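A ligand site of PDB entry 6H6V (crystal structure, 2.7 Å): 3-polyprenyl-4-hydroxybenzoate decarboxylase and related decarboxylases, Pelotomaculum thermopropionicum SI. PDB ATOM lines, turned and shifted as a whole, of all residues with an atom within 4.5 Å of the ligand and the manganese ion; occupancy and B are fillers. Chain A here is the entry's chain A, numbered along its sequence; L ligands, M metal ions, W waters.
An oxygen (O7) of the ligand is in hydrogen-bond range of the backbone NH (N) of His 169, at 2.9 Å. NH2 of Arg 168 lies within hydrogen-bond range of O4 of the ligand. An oxygen (O1) of the ligand lies within hydrogen-bond range of the backbone NH of Leu 166 (2.7 Å). The backbone NH of Ile 150 sits at hydrogen-bond distance from an oxygen (O3) of the ligand, at 2.9 Å. O of Ile 150 lies within hydrogen-bond range of O3 of the ligand (2.7 Å). O2 of the ligand lies within hydrogen-bond range of N of Arg 152, at 2.9 Å. O of Leu 164 is in hydrogen-bond range of N2 of the ligand (2.9 Å). OE1 of Gln 201 lies within hydrogen-bond range of O3 of the ligand, 3.2 Å away. O of Ser 200 lies within hydrogen-bond range of O5 of the ligand, 3.2 Å away.
The side-chain carboxylate of Glu 210 is in hydrogen-bond range of the backbone NH of Val 148 (2.9 Å). O of Leu 164 lies within hydrogen-bond range of ND1 of His 151 (3.0 Å). The side-chain amide oxygen (OE1) of Gln 201 is in hydrogen-bond range of the side-chain hydroxyl (OG) of Ser 200 (3.4 Å). A ring nitrogen (NE2) of His 151 sits at hydrogen-bond distance from the side-chain hydroxyl (OG) of Ser 149.
Residues that only touch the ligand: His 296, His 151, Ser 149, Leu 299, Val 148, Ile 165 and Leu 170. Hydrophobic or aromatic side chains that line the ligand: Ile 150, His 151, Leu 164, Leu 166, His 169, His 296 and Leu 299. Within 4 Å of the ligand: Asn 147, Val 148, Ser 149, Ile 150, His 151, Arg 152, Leu 164, Ile 165, Leu 166, Arg 168, His 169, Leu 170, Ser 200, Gln 201, Glu 210, His 296 and Leu 299. The nearest printed residue that does not touch the ligand is Ala 202 (4.003 Å).
Within 4 Å of the manganese ion: Asn 147, His 169 and Glu 210.
The manganese ion is bound by ND1 of His 169 (2.1 Å), OD1 of Asn 147 (2.2 Å), OE2 of Glu 210 (2.2 Å), O9 of the ligand (2.2 Å) and water W2 (2.3 Å). The manganese ion has five donor atoms within binding distance.
Water W2 bridges O8 of the ligand (2.7 Å) and O of Ala 202 (3.0 Å). Water W5 lies within hydrogen-bond range of O7 of the ligand (2.4 Å), N of Leu 170 (3.3 Å) and OG of Ser 149 (3.4 Å). Water W1 bridges an oxygen (O1) of the ligand (2.7 Å) and the guanidinium group (NE) of Arg 168 (3.2 Å).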
ATOM      1  N   THR A 132     -14.916  21.549  12.527  1.00  0.00           N
ATOM      2  CA  THR A 132     -14.127  20.405  12.973  1.00  0.00           C
ATOM      3  C   THR A 132     -13.310  19.725  11.893  1.00  0.00           C
ATOM      4  O   THR A 132     -12.397  18.960  12.220  1.00  0.00           O
ATOM      5  CB  THR A 132     -15.034  19.340  13.619  1.00  0.00           C
ATOM      6  OG1 THR A 132     -16.084  18.950  12.713  1.00  0.00           O
ATOM      7  CG2 THR A 132     -15.625  19.860  14.905  1.00  0.00           C
ATOM      8  N   ASN A 147       2.695  24.342   5.372  1.00  0.00           N
ATOM      9  CA  ASN A 147       2.312  23.311   6.322  1.00  0.00           C
ATOM     10  C   ASN A 147       0.796  23.158   6.257  1.00  0.00           C
ATOM     11  O   ASN A 147       0.088  24.087   5.922  1.00  0.00           O
ATOM     12  CB  ASN A 147       2.739  23.709   7.733  1.00  0.00           C
ATOM     13  CG  ASN A 147       2.582  22.575   8.741  1.00  0.00           C
ATOM     14  OD1 ASN A 147       3.430  21.712   8.872  1.00  0.00           O
ATOM     15  ND2 ASN A 147       1.496  22.615   9.482  1.00  0.00           N
ATOM     16  N   VAL A 148       0.333  21.953   6.574  1.00  0.00           N
ATOM     17  CA  VAL A 148      -1.076  21.647   6.705  1.00  0.00           C
ATOM     18  C   VAL A 148      -1.297  20.936   8.037  1.00  0.00           C
ATOM     19  O   VAL A 148      -0.532  20.039   8.391  1.00  0.00           O
ATOM     20  CB  VAL A 148      -1.585  20.744   5.554  1.00  0.00           C
ATOM     21  CG1 VAL A 148      -3.103  20.657   5.565  1.00  0.00           C
ATOM     22  CG2 VAL A 148      -1.116  21.269   4.222  1.00  0.00           C
ATOM     23  N   SER A 149      -2.332  21.339   8.755  1.00  0.00           N
ATOM     24  CA  SER A 149      -2.768  20.681   9.987  1.00  0.00           C
ATOM     25  C   SER A 149      -4.245  20.951  10.164  1.00  0.00           C
ATOM     26  O   SER A 149      -4.772  21.837   9.539  1.00  0.00           O
ATOM     27  CB  SER A 149      -1.990  21.203  11.202  1.00  0.00           C
ATOM     28  OG  SER A 149      -1.850  22.623  11.202  1.00  0.00           O
ATOM     29  N   ILE A 150      -4.903  20.201  11.021  1.00  0.00           N
ATOM     30  CA  ILE A 150      -6.311  20.381  11.324  1.00  0.00           C
ATOM     31  C   ILE A 150      -6.444  20.948  12.731  1.00  0.00           C
ATOM     32  O   ILE A 150      -5.793  20.468  13.647  1.00  0.00           O
ATOM     33  CB  ILE A 150      -7.089  19.066  11.222  1.00  0.00           C
ATOM     34  CG1 ILE A 150      -6.987  18.492   9.801  1.00  0.00           C
ATOM     35  CG2 ILE A 150      -8.550  19.298  11.592  1.00  0.00           C
ATOM     36  CD1 ILE A 150      -7.649  17.147   9.600  1.00  0.00           C
ATOM     37  N   HIS A 151      -7.284  21.956  12.916  1.00  0.00           N
ATOM     38  CA  HIS A 151      -7.475  22.622  14.197  1.00  0.00           C
ATOM     39  C   HIS A 151      -8.922  22.938  14.404  1.00  0.00           C
ATOM     40  O   HIS A 151      -9.599  23.382  13.462  1.00  0.00           O
ATOM     41  CB  HIS A 151      -6.700  23.917  14.272  1.00  0.00           C
ATOM     42  CG  HIS A 151      -5.241  23.753  14.019  1.00  0.00           C
ATOM     43  ND1 HIS A 151      -4.324  23.692  15.050  1.00  0.00           N
ATOM     44  CD2 HIS A 151      -4.546  23.575  12.868  1.00  0.00           C
ATOM     45  CE1 HIS A 151      -3.118  23.505  14.529  1.00  0.00           C
ATOM     46  NE2 HIS A 151      -3.236  23.432  13.209  1.00  0.00           N
ATOM     47  N   ARG A 152      -9.414  22.729  15.624  1.00  0.00           N
ATOM     48  CA  ARG A 152     -10.785  23.076  15.947  1.00  0.00           C
ATOM     49  C   ARG A 152     -10.949  24.601  15.932  1.00  0.00           C
ATOM     50  O   ARG A 152     -10.046  25.346  16.337  1.00  0.00           O
ATOM     51  CB  ARG A 152     -11.186  22.482  17.300  1.00  0.00           C
ATOM     52  CG  ARG A 152     -10.613  23.154  18.533  1.00  0.00           C
ATOM     53  CD  ARG A 152     -11.109  22.471  19.780  1.00  0.00           C
ATOM     54  NE  ARG A 152     -10.703  23.179  20.981  1.00  0.00           N
ATOM     55  CZ  ARG A 152     -10.243  22.618  22.091  1.00  0.00           C
ATOM     56  NH1 ARG A 152     -10.051  21.298  22.211  1.00  0.00           N
ATOM     57  NH2 ARG A 152      -9.897  23.404  23.098  1.00  0.00           N
ATOM     58  N   LEU A 164      -7.480  26.451  18.625  1.00  0.00           N
ATOM     59  CA  LEU A 164      -6.507  25.740  19.469  1.00  0.00           C
ATOM     60  C   LEU A 164      -5.309  25.396  18.611  1.00  0.00           C
ATOM     61  O   LEU A 164      -5.431  24.654  17.634  1.00  0.00           O
ATOM     62  CB  LEU A 164      -7.078  24.462  20.048  1.00  0.00           C
ATOM     63  CG  LEU A 164      -6.124  23.610  20.883  1.00  0.00           C
ATOM     64  CD1 LEU A 164      -5.815  24.288  22.196  1.00  0.00           C
ATOM     65  CD2 LEU A 164      -6.671  22.216  21.096  1.00  0.00           C
ATOM     66  N   ILE A 165      -4.153  25.948  18.982  1.00  0.00           N
ATOM     67  CA  ILE A 165      -2.904  25.613  18.318  1.00  0.00           C
ATOM     68  C   ILE A 165      -2.003  24.936  19.360  1.00  0.00           C
ATOM     69  O   ILE A 165      -1.410  25.605  20.217  1.00  0.00           O
ATOM     70  CB  ILE A 165      -2.211  26.853  17.713  1.00  0.00           C
ATOM     71  CG1 ILE A 165      -3.220  27.751  16.982  1.00  0.00           C
ATOM     72  CG2 ILE A 165      -1.101  26.424  16.760  1.00  0.00           C
ATOM     73  CD1 ILE A 165      -2.598  28.941  16.272  1.00  0.00           C
ATOM     74  N   LEU A 166      -1.901  23.602  19.277  1.00  0.00           N
ATOM     75  CA  LEU A 166      -0.910  22.864  20.052  1.00  0.00           C
ATOM     76  C   LEU A 166       0.476  23.151  19.489  1.00  0.00           C
ATOM     77  O   LEU A 166       0.607  23.545  18.315  1.00  0.00           O
ATOM     78  CB  LEU A 166      -1.202  21.351  20.028  1.00  0.00           C
ATOM     79  CG  LEU A 166      -2.538  20.888  20.625  1.00  0.00           C
ATOM     80  CD1 LEU A 166      -2.858  19.461  20.220  1.00  0.00           C
ATOM     81  CD2 LEU A 166      -2.554  21.009  22.133  1.00  0.00           C
ATOM     82  N   ARG A 168       3.199  22.565  17.655  1.00  0.00           N
ATOM     83  CA  ARG A 168       3.892  21.838  16.581  1.00  0.00           C
ATOM     84  C   ARG A 168       4.155  22.884  15.479  1.00  0.00           C
ATOM     85  O   ARG A 168       4.607  23.959  15.802  1.00  0.00           O
ATOM     86  CB  ARG A 168       3.127  20.589  16.089  1.00  0.00           C
ATOM     87  CG  ARG A 168       3.215  19.354  16.986  1.00  0.00           C
ATOM     88  CD  ARG A 168       2.125  19.363  18.070  1.00  0.00           C
ATOM     89  NE  ARG A 168       0.837  18.833  17.584  1.00  0.00           N
ATOM     90  CZ  ARG A 168       0.174  17.763  18.053  1.00  0.00           C
ATOM     91  NH1 ARG A 168       0.631  17.047  19.080  1.00  0.00           N
ATOM     92  NH2 ARG A 168      -0.975  17.450  17.499  1.00  0.00           N
ATOM     93  N   HIS A 169       3.881  22.592  14.195  1.00  0.00           N
ATOM     94  CA  HIS A 169       4.394  23.427  13.115  1.00  0.00           C
ATOM     95  C   HIS A 169       3.637  24.741  12.948  1.00  0.00           C
ATOM     96  O   HIS A 169       4.245  25.773  12.670  1.00  0.00           O
ATOM     97  CB  HIS A 169       4.410  22.663  11.792  1.00  0.00           C
ATOM     98  CG  HIS A 169       5.375  21.513  11.774  1.00  0.00           C
ATOM     99  ND1 HIS A 169       5.296  20.483  10.864  1.00  0.00           N
ATOM    100  CD2 HIS A 169       6.443  21.236  12.568  1.00  0.00           C
ATOM    101  CE1 HIS A 169       6.275  19.623  11.087  1.00  0.00           C
ATOM    102  NE2 HIS A 169       6.982  20.057  12.115  1.00  0.00           N
ATOM    103  N   LEU A 170       2.317  24.735  13.085  1.00  0.00           N
ATOM    104  CA  LEU A 170       1.584  25.981  12.963  1.00  0.00           C
ATOM    105  C   LEU A 170       2.007  26.952  14.061  1.00  0.00           C
ATOM    106  O   LEU A 170       2.111  28.138  13.819  1.00  0.00           O
ATOM    107  CB  LEU A 170       0.070  25.781  12.985  1.00  0.00           C
ATOM    108  CG  LEU A 170      -0.755  27.052  12.717  1.00  0.00           C
ATOM    109  CD1 LEU A 170      -0.405  27.694  11.372  1.00  0.00           C
ATOM    110  CD2 LEU A 170      -2.242  26.720  12.791  1.00  0.00           C
ATOM    111  N   SER A 200      -2.741  15.604   6.213  1.00  0.00           N
ATOM    112  CA  SER A 200      -2.596  16.712   7.157  1.00  0.00           C
ATOM    113  C   SER A 200      -2.110  16.221   8.517  1.00  0.00           C
ATOM    114  O   SER A 200      -1.483  16.983   9.248  1.00  0.00           O
ATOM    115  CB  SER A 200      -3.904  17.474   7.352  1.00  0.00           C
ATOM    116  OG  SER A 200      -4.860  16.658   8.027  1.00  0.00           O
ATOM    117  N   GLN A 201      -2.393  14.960   8.831  1.00  0.00           N
ATOM    118  CA  GLN A 201      -1.923  14.317  10.065  1.00  0.00           C
ATOM    119  C   GLN A 201      -0.552  13.678   9.977  1.00  0.00           C
ATOM    120  O   GLN A 201      -0.063  13.169  10.974  1.00  0.00           O
ATOM    121  CB  GLN A 201      -2.891  13.220  10.479  1.00  0.00           C
ATOM    122  CG  GLN A 201      -4.304  13.741  10.680  1.00  0.00           C
ATOM    123  CD  GLN A 201      -4.325  14.851  11.675  1.00  0.00           C
ATOM    124  OE1 GLN A 201      -4.547  16.000  11.301  1.00  0.00           O
ATOM    125  NE2 GLN A 201      -4.089  14.519  12.910  1.00  0.00           N
ATOM    126  N   ALA A 202       0.062  13.647   8.800  1.00  0.00           N
ATOM    127  CA  ALA A 202       1.400  13.075   8.671  1.00  0.00           C
ATOM    128  C   ALA A 202       2.348  13.880   9.525  1.00  0.00           C
ATOM    129  O   ALA A 202       2.270  15.123   9.612  1.00  0.00           O
ATOM    130  CB  ALA A 202       1.868  13.056   7.232  1.00  0.00           C
ATOM    131  N   THR A 204       6.130  14.746  10.469  1.00  0.00           N
ATOM    132  CA  THR A 204       7.354  14.825   9.644  1.00  0.00           C
ATOM    133  C   THR A 204       8.352  15.863  10.127  1.00  0.00           C
ATOM    134  O   THR A 204       8.088  16.643  11.045  1.00  0.00           O
ATOM    135  CB  THR A 204       7.035  15.217   8.174  1.00  0.00           C
ATOM    136  OG1 THR A 204       6.650  16.599   8.096  1.00  0.00           O
ATOM    137  CG2 THR A 204       5.913  14.360   7.606  1.00  0.00           C
ATOM    138  N   VAL A 208       8.557  19.889   5.393  1.00  0.00           N
ATOM    139  CA  VAL A 208       7.807  19.178   4.337  1.00  0.00           C
ATOM    140  C   VAL A 208       6.319  19.551   4.244  1.00  0.00           C
ATOM    141  O   VAL A 208       5.604  19.643   5.237  1.00  0.00           O
ATOM    142  CB  VAL A 208       8.057  17.637   4.240  1.00  0.00           C
ATOM    143  CG1 VAL A 208       9.209  17.200   5.129  1.00  0.00           C
ATOM    144  CG2 VAL A 208       6.812  16.797   4.477  1.00  0.00           C
ATOM    145  N   GLU A 210       2.633  18.909   3.463  1.00  0.00           N
ATOM    146  CA  GLU A 210       1.683  17.799   3.521  1.00  0.00           C
ATOM    147  C   GLU A 210       0.740  17.722   2.324  1.00  0.00           C
ATOM    148  O   GLU A 210       0.195  16.645   2.038  1.00  0.00           O
ATOM    149  CB  GLU A 210       0.869  17.856   4.812  1.00  0.00           C
ATOM    150  CG  GLU A 210       1.728  17.532   6.036  1.00  0.00           C
ATOM    151  CD  GLU A 210       2.235  18.786   6.780  1.00  0.00           C
ATOM    152  OE1 GLU A 210       2.254  19.883   6.184  1.00  0.00           O
ATOM    153  OE2 GLU A 210       2.608  18.661   7.967  1.00  0.00           O
ATOM    154  N   ILE A 289     -16.614  16.594  11.139  1.00  0.00           N
ATOM    155  CA  ILE A 289     -16.101  15.416  11.831  1.00  0.00           C
ATOM    156  C   ILE A 289     -16.642  15.499  13.261  1.00  0.00           C
ATOM    157  O   ILE A 289     -16.365  16.467  13.993  1.00  0.00           O
ATOM    158  CB  ILE A 289     -14.564  15.371  11.836  1.00  0.00           C
ATOM    159  CG1 ILE A 289     -14.027  15.161  10.425  1.00  0.00           C
ATOM    160  CG2 ILE A 289     -14.069  14.212  12.700  1.00  0.00           C
ATOM    161  CD1 ILE A 289     -12.519  15.354  10.267  1.00  0.00           C
ATOM    162  N   HIS A 296     -12.708  10.716  13.221  1.00  0.00           N
ATOM    163  CA  HIS A 296     -11.791  11.514  14.020  1.00  0.00           C
ATOM    164  C   HIS A 296     -10.603  10.711  14.493  1.00  0.00           C
ATOM    165  O   HIS A 296      -9.456  11.124  14.340  1.00  0.00           O
ATOM    166  CB  HIS A 296     -12.517  12.109  15.246  1.00  0.00           C
ATOM    167  CG  HIS A 296     -11.701  13.071  16.042  1.00  0.00           C
ATOM    168  ND1 HIS A 296     -12.179  13.672  17.178  1.00  0.00           N
ATOM    169  CD2 HIS A 296     -10.441  13.545  15.884  1.00  0.00           C
ATOM    170  CE1 HIS A 296     -11.260  14.469  17.692  1.00  0.00           C
ATOM    171  NE2 HIS A 296     -10.202  14.430  16.900  1.00  0.00           N
ATOM    172  N   LEU A 299      -8.073   9.167  11.686  1.00  0.00           N
ATOM    173  CA  LEU A 299      -7.246  10.134  10.961  1.00  0.00           C
ATOM    174  C   LEU A 299      -5.880  10.236  11.622  1.00  0.00           C
ATOM    175  O   LEU A 299      -4.845  10.066  10.977  1.00  0.00           O
ATOM    176  CB  LEU A 299      -7.880  11.523  10.888  1.00  0.00           C
ATOM    177  CG  LEU A 299      -8.900  11.748   9.789  1.00  0.00           C
ATOM    178  CD1 LEU A 299      -9.556  13.102   9.946  1.00  0.00           C
ATOM    179  CD2 LEU A 299      -8.294  11.626   8.416  1.00  0.00           C
ATOM    180  N   GLY A 300      -5.891  10.512  12.929  1.00  0.00           N
ATOM    181  CA  GLY A 300      -4.670  10.518  13.722  1.00  0.00           C
ATOM    182  C   GLY A 300      -4.100   9.126  13.947  1.00  0.00           C
ATOM    183  O   GLY A 300      -2.888   8.951  13.970  1.00  0.00           O
HETATM  184  N1  LIG L   1      -4.228  20.015  16.695  1.00  0.00           N
HETATM  185  C1  LIG L   1      -4.273  21.171  17.400  1.00  0.00           C
HETATM  186  O1  LIG L   1      -3.203  21.720  17.762  1.00  0.00           O
HETATM  187  N2  LIG L   1      -5.436  21.738  17.740  1.00  0.00           N
HETATM  188  C2  LIG L   1      -6.599  21.209  17.375  1.00  0.00           C
HETATM  189  O2  LIG L   1      -7.650  21.788  17.690  1.00  0.00           O
HETATM  190  C3  LIG L   1      -6.631  19.951  16.598  1.00  0.00           C
HETATM  191  N3  LIG L   1      -7.766  19.382  16.203  1.00  0.00           N
HETATM  192  C4  LIG L   1      -7.744  18.244  15.456  1.00  0.00           C
HETATM  193  C5  LIG L   1      -8.928  17.668  15.015  1.00  0.00           C
HETATM  194  C6  LIG L   1      -8.940  16.515  14.250  1.00  0.00           C
HETATM  195  C7  LIG L   1     -10.270  15.962  13.811  1.00  0.00           C
HETATM  196  C8  LIG L   1      -7.676  15.844  13.848  1.00  0.00           C
HETATM  197  C9  LIG L   1      -7.692  14.552  13.038  1.00  0.00           C
HETATM  198  C10 LIG L   1      -6.495  16.411  14.284  1.00  0.00           C
HETATM  199  C11 LIG L   1      -6.465  17.576  15.061  1.00  0.00           C
HETATM  200  N4  LIG L   1      -5.257  18.190  15.504  1.00  0.00           N
HETATM  201  C12 LIG L   1      -5.339  19.376  16.264  1.00  0.00           C
HETATM  202  C13 LIG L   1      -3.936  17.591  15.284  1.00  0.00           C
HETATM  203  C14 LIG L   1      -3.051  18.166  14.245  1.00  0.00           C
HETATM  204  O3  LIG L   1      -3.896  18.547  13.148  1.00  0.00           O
HETATM  205  C15 LIG L   1      -2.042  17.079  13.912  1.00  0.00           C
HETATM  206  O4  LIG L   1      -1.359  16.670  15.090  1.00  0.00           O
HETATM  207  C16 LIG L   1      -1.096  17.570  12.861  1.00  0.00           C
HETATM  208  O5  LIG L   1      -0.436  16.435  12.254  1.00  0.00           O
HETATM  209  C17 LIG L   1      -0.058  18.564  13.358  1.00  0.00           C
HETATM  210  O6  LIG L   1       0.684  18.863  12.173  1.00  0.00           O
HETATM  211  P1  LIG L   1       2.090  19.673  12.203  1.00  0.00           P
HETATM  212  O7  LIG L   1       1.840  20.831  13.156  1.00  0.00           O
HETATM  213  O8  LIG L   1       3.138  18.702  12.699  1.00  0.00           O
HETATM  214  O9  LIG L   1       2.380  20.030  10.741  1.00  0.00           O
HETATM  215 MN    MN M   1       4.062  19.688   9.311  1.00  0.00          MN
HETATM  216  O   HOH W   1      -1.092  20.964  16.233  1.00  0.00           O
HETATM  217  O   HOH W   2       3.854  17.587  10.300  1.00  0.00           O
HETATM  218  O   HOH W   3     -11.109  18.908  16.958  1.00  0.00           O
HETATM  219  O   HOH W   4       5.123  18.181  14.797  1.00  0.00           O
HETATM  220  O   HOH W   5       0.157  22.440  13.907  1.00  0.00           O
